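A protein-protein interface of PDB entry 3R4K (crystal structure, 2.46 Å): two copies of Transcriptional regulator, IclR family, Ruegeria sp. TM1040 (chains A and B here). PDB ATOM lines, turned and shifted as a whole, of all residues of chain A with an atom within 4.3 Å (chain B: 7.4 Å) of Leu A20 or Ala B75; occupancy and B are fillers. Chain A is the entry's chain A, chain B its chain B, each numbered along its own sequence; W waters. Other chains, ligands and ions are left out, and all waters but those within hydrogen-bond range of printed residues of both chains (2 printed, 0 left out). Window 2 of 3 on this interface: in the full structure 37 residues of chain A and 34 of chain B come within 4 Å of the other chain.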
ATOM      1  N   PHE A  15     -14.049 -14.890  12.536  1.00  0.00           N
ATOM      2  CA  PHE A  15     -14.326 -13.745  11.684  1.00  0.00           C
ATOM      3  C   PHE A  15     -13.030 -13.018  11.412  1.00  0.00           C
ATOM      4  O   PHE A  15     -12.241 -12.811  12.336  1.00  0.00           O
ATOM      5  CB  PHE A  15     -15.323 -12.798  12.361  1.00  0.00           C
ATOM      6  CG  PHE A  15     -16.731 -13.309  12.400  1.00  0.00           C
ATOM      7  CD1 PHE A  15     -17.574 -13.160  11.303  1.00  0.00           C
ATOM      8  CD2 PHE A  15     -17.229 -13.930  13.541  1.00  0.00           C
ATOM      9  CE1 PHE A  15     -18.879 -13.641  11.339  1.00  0.00           C
ATOM     10  CE2 PHE A  15     -18.543 -14.405  13.579  1.00  0.00           C
ATOM     11  CZ  PHE A  15     -19.355 -14.265  12.476  1.00  0.00           C
ATOM     12  N   ASN A  16     -12.793 -12.643  10.150  1.00  0.00           N
ATOM     13  CA  ASN A  16     -11.611 -11.884   9.718  1.00  0.00           C
ATOM     14  C   ASN A  16     -12.005 -11.115   8.448  1.00  0.00           C
ATOM     15  O   ASN A  16     -13.086 -11.350   7.922  1.00  0.00           O
ATOM     16  CB  ASN A  16     -10.368 -12.799   9.521  1.00  0.00           C
ATOM     17  CG  ASN A  16     -10.546 -13.948   8.562  1.00  0.00           C
ATOM     18  OD1 ASN A  16     -10.627 -13.766   7.355  1.00  0.00           O
ATOM     19  ND2 ASN A  16     -10.550 -15.165   9.069  1.00  0.00           N
ATOM     20  N   HIS A  17     -11.185 -10.169   7.989  1.00  0.00           N
ATOM     21  CA  HIS A  17     -11.509  -9.362   6.810  1.00  0.00           C
ATOM     22  C   HIS A  17     -11.781 -10.217   5.561  1.00  0.00           C
ATOM     23  O   HIS A  17     -12.460  -9.722   4.662  1.00  0.00           O
ATOM     24  CB  HIS A  17     -10.415  -8.319   6.524  1.00  0.00           C
ATOM     25  CG  HIS A  17     -10.401  -7.176   7.496  1.00  0.00           C
ATOM     26  ND1 HIS A  17     -11.215  -6.075   7.323  1.00  0.00           N
ATOM     27  CD2 HIS A  17      -9.681  -7.014   8.629  1.00  0.00           C
ATOM     28  CE1 HIS A  17     -10.954  -5.267   8.337  1.00  0.00           C
ATOM     29  NE2 HIS A  17     -10.031  -5.786   9.148  1.00  0.00           N
ATOM     30  N   GLY A  18     -11.294 -11.475   5.537  1.00  0.00           N
ATOM     31  CA  GLY A  18     -11.534 -12.427   4.452  1.00  0.00           C
ATOM     32  C   GLY A  18     -12.746 -13.312   4.679  1.00  0.00           C
ATOM     33  O   GLY A  18     -13.153 -14.049   3.775  1.00  0.00           O
ATOM     34  N   ARG A  19     -13.332 -13.247   5.895  1.00  0.00           N
ATOM     35  CA  ARG A  19     -14.502 -14.033   6.307  1.00  0.00           C
ATOM     36  C   ARG A  19     -15.366 -13.199   7.265  1.00  0.00           C
ATOM     37  O   ARG A  19     -15.281 -13.352   8.484  1.00  0.00           O
ATOM     38  CB  ARG A  19     -14.018 -15.333   6.960  1.00  0.00           C
ATOM     39  CG  ARG A  19     -15.078 -16.421   7.087  1.00  0.00           C
ATOM     40  CD  ARG A  19     -14.439 -17.757   7.419  1.00  0.00           C
ATOM     41  NE  ARG A  19     -13.497 -17.665   8.540  1.00  0.00           N
ATOM     42  CZ  ARG A  19     -12.513 -18.527   8.767  1.00  0.00           C
ATOM     43  NH1 ARG A  19     -12.335 -19.566   7.962  1.00  0.00           N
ATOM     44  NH2 ARG A  19     -11.709 -18.367   9.809  1.00  0.00           N
ATOM     45  N   LEU A  20     -16.157 -12.275   6.709  1.00  0.00           N
ATOM     46  CA  LEU A  20     -16.974 -11.336   7.490  1.00  0.00           C
ATOM     47  C   LEU A  20     -18.340 -11.907   7.837  1.00  0.00           C
ATOM     48  O   LEU A  20     -18.966 -11.455   8.796  1.00  0.00           O
ATOM     49  CB  LEU A  20     -17.131 -10.000   6.740  1.00  0.00           C
ATOM     50  CG  LEU A  20     -15.871  -9.204   6.481  1.00  0.00           C
ATOM     51  CD1 LEU A  20     -16.124  -8.136   5.447  1.00  0.00           C
ATOM     52  CD2 LEU A  20     -15.294  -8.643   7.760  1.00  0.00           C
ATOM     53  N   GLU A  21     -18.787 -12.906   7.073  1.00  0.00           N
ATOM     54  CA  GLU A  21     -20.049 -13.599   7.285  1.00  0.00           C
ATOM     55  C   GLU A  21     -19.799 -15.099   7.349  1.00  0.00           C
ATOM     56  O   GLU A  21     -19.115 -15.651   6.488  1.00  0.00           O
ATOM     57  CB  GLU A  21     -21.072 -13.263   6.190  1.00  0.00           C
ATOM     58  CG  GLU A  21     -21.602 -11.842   6.263  1.00  0.00           C
ATOM     59  CD  GLU A  21     -22.613 -11.465   5.194  1.00  0.00           C
ATOM     60  OE1 GLU A  21     -23.291 -12.372   4.655  1.00  0.00           O
ATOM     61  OE2 GLU A  21     -22.738 -10.251   4.907  1.00  0.00           O
ATOM     62  N   TYR A  60     -24.171 -15.370  10.023  1.00  0.00           N
ATOM     63  CA  TYR A  60     -23.914 -14.363  11.038  1.00  0.00           C
ATOM     64  C   TYR A  60     -22.805 -13.444  10.613  1.00  0.00           C
ATOM     65  O   TYR A  60     -21.879 -13.855   9.907  1.00  0.00           O
ATOM     66  CB  TYR A  60     -23.522 -14.998  12.377  1.00  0.00           C
ATOM     67  CG  TYR A  60     -24.511 -15.980  12.965  1.00  0.00           C
ATOM     68  CD1 TYR A  60     -25.553 -15.547  13.783  1.00  0.00           C
ATOM     69  CD2 TYR A  60     -24.339 -17.354  12.803  1.00  0.00           C
ATOM     70  CE1 TYR A  60     -26.433 -16.450  14.374  1.00  0.00           C
ATOM     71  CE2 TYR A  60     -25.206 -18.267  13.399  1.00  0.00           C
ATOM     72  CZ  TYR A  60     -26.245 -17.810  14.191  1.00  0.00           C
ATOM     73  OH  TYR A  60     -27.093 -18.704  14.790  1.00  0.00           O
ATOM     74  N   ARG A  61     -22.887 -12.206  11.069  1.00  0.00           N
ATOM     75  CA  ARG A  61     -21.853 -11.198  10.901  1.00  0.00           C
ATOM     76  C   ARG A  61     -21.716 -10.486  12.238  1.00  0.00           C
ATOM     77  O   ARG A  61     -22.584 -10.639  13.112  1.00  0.00           O
ATOM     78  CB  ARG A  61     -22.142 -10.240   9.744  1.00  0.00           C
ATOM     79  CG  ARG A  61     -23.333  -9.336   9.957  1.00  0.00           C
ATOM     80  CD  ARG A  61     -23.511  -8.449   8.765  1.00  0.00           C
ATOM     81  NE  ARG A  61     -24.452  -7.371   9.050  1.00  0.00           N
ATOM     82  CZ  ARG A  61     -24.922  -6.532   8.134  1.00  0.00           C
ATOM     83  NH1 ARG A  61     -24.561  -6.657   6.860  1.00  0.00           N
ATOM     84  NH2 ARG A  61     -25.771  -5.570   8.479  1.00  0.00           N
ATOM     85  N   LEU B  69     -12.806  -6.393  16.294  1.00  0.00           N
ATOM     86  CA  LEU B  69     -14.213  -6.662  16.007  1.00  0.00           C
ATOM     87  C   LEU B  69     -14.924  -5.439  15.426  1.00  0.00           C
ATOM     88  O   LEU B  69     -15.752  -5.595  14.525  1.00  0.00           O
ATOM     89  CB  LEU B  69     -14.958  -7.148  17.256  1.00  0.00           C
ATOM     90  CG  LEU B  69     -14.441  -8.419  17.936  1.00  0.00           C
ATOM     91  CD1 LEU B  69     -15.338  -8.792  19.076  1.00  0.00           C
ATOM     92  CD2 LEU B  69     -14.315  -9.581  16.986  1.00  0.00           C
ATOM     93  N   ALA B  70     -14.587  -4.228  15.902  1.00  0.00           N
ATOM     94  CA  ALA B  70     -15.207  -3.015  15.357  1.00  0.00           C
ATOM     95  C   ALA B  70     -14.784  -2.810  13.902  1.00  0.00           C
ATOM     96  O   ALA B  70     -15.605  -2.397  13.086  1.00  0.00           O
ATOM     97  CB  ALA B  70     -14.833  -1.813  16.191  1.00  0.00           C
ATOM     98  N   ALA B  71     -13.521  -3.163  13.566  1.00  0.00           N
ATOM     99  CA  ALA B  71     -12.989  -3.048  12.206  1.00  0.00           C
ATOM    100  C   ALA B  71     -13.702  -3.986  11.262  1.00  0.00           C
ATOM    101  O   ALA B  71     -13.948  -3.609  10.123  1.00  0.00           O
ATOM    102  CB  ALA B  71     -11.511  -3.335  12.192  1.00  0.00           C
ATOM    103  N   LEU B  72     -14.044  -5.199  11.733  1.00  0.00           N
ATOM    104  CA  LEU B  72     -14.783  -6.184  10.928  1.00  0.00           C
ATOM    105  C   LEU B  72     -16.242  -5.741  10.750  1.00  0.00           C
ATOM    106  O   LEU B  72     -16.771  -5.838   9.647  1.00  0.00           O
ATOM    107  CB  LEU B  72     -14.697  -7.588  11.537  1.00  0.00           C
ATOM    108  CG  LEU B  72     -13.296  -8.189  11.684  1.00  0.00           C
ATOM    109  CD1 LEU B  72     -13.340  -9.491  12.435  1.00  0.00           C
ATOM    110  CD2 LEU B  72     -12.571  -8.290  10.352  1.00  0.00           C
ATOM    111  N   ARG B  73     -16.848  -5.177  11.813  1.00  0.00           N
ATOM    112  CA  ARG B  73     -18.192  -4.607  11.772  1.00  0.00           C
ATOM    113  C   ARG B  73     -18.225  -3.481  10.748  1.00  0.00           C
ATOM    114  O   ARG B  73     -19.139  -3.431   9.927  1.00  0.00           O
ATOM    115  CB  ARG B  73     -18.641  -4.108  13.180  1.00  0.00           C
ATOM    116  CG  ARG B  73     -19.963  -3.323  13.228  1.00  0.00           C
ATOM    117  CD  ARG B  73     -21.148  -4.095  12.666  1.00  0.00           C
ATOM    118  NE  ARG B  73     -22.369  -3.299  12.576  1.00  0.00           N
ATOM    119  CZ  ARG B  73     -23.562  -3.801  12.254  1.00  0.00           C
ATOM    120  NH1 ARG B  73     -23.702  -5.100  12.023  1.00  0.00           N
ATOM    121  NH2 ARG B  73     -24.631  -3.019  12.219  1.00  0.00           N
ATOM    122  N   GLU B  74     -17.205  -2.614  10.759  1.00  0.00           N
ATOM    123  CA  GLU B  74     -17.088  -1.488   9.835  1.00  0.00           C
ATOM    124  C   GLU B  74     -16.822  -1.940   8.401  1.00  0.00           C
ATOM    125  O   GLU B  74     -17.269  -1.273   7.487  1.00  0.00           O
ATOM    126  CB  GLU B  74     -16.025  -0.505  10.317  1.00  0.00           C
ATOM    127  CG  GLU B  74     -16.626   0.517  11.268  1.00  0.00           C
ATOM    128  CD  GLU B  74     -17.417   1.647  10.614  1.00  0.00           C
ATOM    129  OE1 GLU B  74     -16.959   2.203   9.587  1.00  0.00           O
ATOM    130  OE2 GLU B  74     -18.480   2.007  11.164  1.00  0.00           O
ATOM    131  N   ALA B  75     -16.150  -3.089   8.194  1.00  0.00           N
ATOM    132  CA  ALA B  75     -15.962  -3.647   6.860  1.00  0.00           C
ATOM    133  C   ALA B  75     -17.317  -4.151   6.346  1.00  0.00           C
ATOM    134  O   ALA B  75     -17.607  -3.984   5.165  1.00  0.00           O
ATOM    135  CB  ALA B  75     -14.945  -4.761   6.891  1.00  0.00           C
ATOM    136  N   SER B  76     -18.170  -4.699   7.243  1.00  0.00           N
ATOM    137  CA  SER B  76     -19.521  -5.131   6.891  1.00  0.00           C
ATOM    138  C   SER B  76     -20.481  -3.928   6.658  1.00  0.00           C
ATOM    139  O   SER B  76     -21.186  -3.902   5.641  1.00  0.00           O
ATOM    140  CB  SER B  76     -20.084  -6.034   7.978  1.00  0.00           C
ATOM    141  OG  SER B  76     -19.375  -7.260   7.978  1.00  0.00           O
ATOM    142  N   VAL B  77     -20.515  -2.944   7.628  1.00  0.00           N
ATOM    143  CA  VAL B  77     -21.381  -1.745   7.612  1.00  0.00           C
ATOM    144  C   VAL B  77     -20.490  -0.516   7.816  1.00  0.00           C
ATOM    145  O   VAL B  77     -20.260  -0.102   8.960  1.00  0.00           O
ATOM    146  CB  VAL B  77     -22.537  -1.832   8.662  1.00  0.00           C
ATOM    147  CG1 VAL B  77     -23.485  -0.649   8.554  1.00  0.00           C
ATOM    148  CG2 VAL B  77     -23.300  -3.157   8.557  1.00  0.00           C
ATOM    149  N   PRO B  78     -19.965   0.074   6.712  1.00  0.00           N
ATOM    150  CA  PRO B  78     -18.986   1.177   6.851  1.00  0.00           C
ATOM    151  C   PRO B  78     -19.588   2.527   7.245  1.00  0.00           C
ATOM    152  O   PRO B  78     -19.307   3.541   6.605  1.00  0.00           O
ATOM    153  CB  PRO B  78     -18.329   1.239   5.468  1.00  0.00           C
ATOM    154  CG  PRO B  78     -19.366   0.701   4.536  1.00  0.00           C
ATOM    155  CD  PRO B  78     -20.122  -0.342   5.302  1.00  0.00           C
ATOM    156  N   ILE B  79     -20.289   2.573   8.370  1.00  0.00           N
ATOM    157  CA  ILE B  79     -20.954   3.797   8.753  1.00  0.00           C
ATOM    158  C   ILE B  79     -19.987   4.883   9.289  1.00  0.00           C
ATOM    159  O   ILE B  79     -20.064   6.012   8.815  1.00  0.00           O
ATOM    160  CB  ILE B  79     -22.166   3.536   9.702  1.00  0.00           C
ATOM    161  CG1 ILE B  79     -22.942   4.834   9.950  1.00  0.00           C
ATOM    162  CG2 ILE B  79     -21.786   2.823  11.007  1.00  0.00           C
ATOM    163  CD1 ILE B  79     -24.365   4.758   9.761  1.00  0.00           C
ATOM    164  N   SER B  81     -16.719   5.153   8.939  1.00  0.00           N
ATOM    165  CA  SER B  81     -15.737   5.438   7.902  1.00  0.00           C
ATOM    166  C   SER B  81     -16.362   6.371   6.862  1.00  0.00           C
ATOM    167  O   SER B  81     -15.729   7.337   6.447  1.00  0.00           O
ATOM    168  CB  SER B  81     -15.273   4.128   7.274  1.00  0.00           C
ATOM    169  OG  SER B  81     -14.427   4.343   6.161  1.00  0.00           O
HETATM  170  O   HOH W   1     -21.407  -7.755   5.322  1.00  0.00           O
HETATM  171  O   HOH W   2     -18.736  -9.054  10.151  1.00  0.00           O
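Of chain B, only Leu B72 (3.7 Å), Ala B75 (3.9 Å) and Ser B76 (3.8 Å) come within 4 Å of Leu A20.
Of chain A, only His A17 (3.98 Å) and Leu A20 (3.9 Å) come within 4 Å of Ala B75.
Of the printed residues of chain B, His A17 touches Ala B71 (3.9 Å), Leu B72 (3.3 Å) and Ala B75 (3.98 Å).
Printed residues of chain A within 4 Å of Val B77: Arg A61 (3.5 Å).
Printed residues of chain A within 4 Å of Ala B71: His A17.
Of the printed residues of chain B, Phe A15 touches Leu B72 (3.5 Å).
Of the printed residues of chain A, Ser B76 touches Leu A20.
Pro B78 touches none of the printed residues of chain A.
The nearest residue of chain B that does not touch Leu A20 is Arg B73 (5.6 Å).
The nearest printed residue of chain A that does not touch Ala B75 is Asn A16 (6.9 Å).
The nearest printed residue of chain A that does not touch Leu B72 is Arg A19 (5.9 Å).
No position is printed for both chains.
The side-chain amide oxygen of Asn A16 is in hydrogen-bond range of the backbone NH of Gly A18, 3.0 Å away.
OD1 of Asn A16 is in hydrogen-bond range of N of Arg A19, at 3.1 Å.
The side-chain hydroxyl (OG) of Ser B76 sits at hydrogen-bond distance from the backbone carbonyl oxygen (O) of Leu B72, 3.4 Å away.
Water W2 bridges O of Leu A20 (2.8 Å) and OG of Ser B76 (2.9 Å).
Water W1 lies within hydrogen-bond range of OE2 of Glu A21 (2.9 Å) and OG of Ser B76 (3.4 Å).
Of the 9 printed residues of chain A, 5 touch a printed residue of chain B.
Printed residues of chain A that touch a printed residue of chain B: Phe A15, Asn A16, His A17, Leu A20 and Arg A61.
Hydrophobic or aromatic side chains of chain A within 4 Å of the printed part of chain B: Phe A15, His A17 and Leu A20.
Of the 12 printed residues of chain B, 6 touch a printed residue of chain A.
Among the printed residues, no Asp or Glu carboxylate lies within 4 Å of a Lys or Arg side-chain nitrogen of the other chain.
Among the printed residues, pairs that only touch across the chains: His A17 with Leu B72, Asn A16 with Leu B72, Arg A61 with Val B77, Phe A15 with Leu B72, Leu A20 with Leu B72, Leu A20 with Ser B76, Arg A61 with Arg B73, Leu A20 with Ala B75, His A17 with Ala B71 and His A17 with Ala B75.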
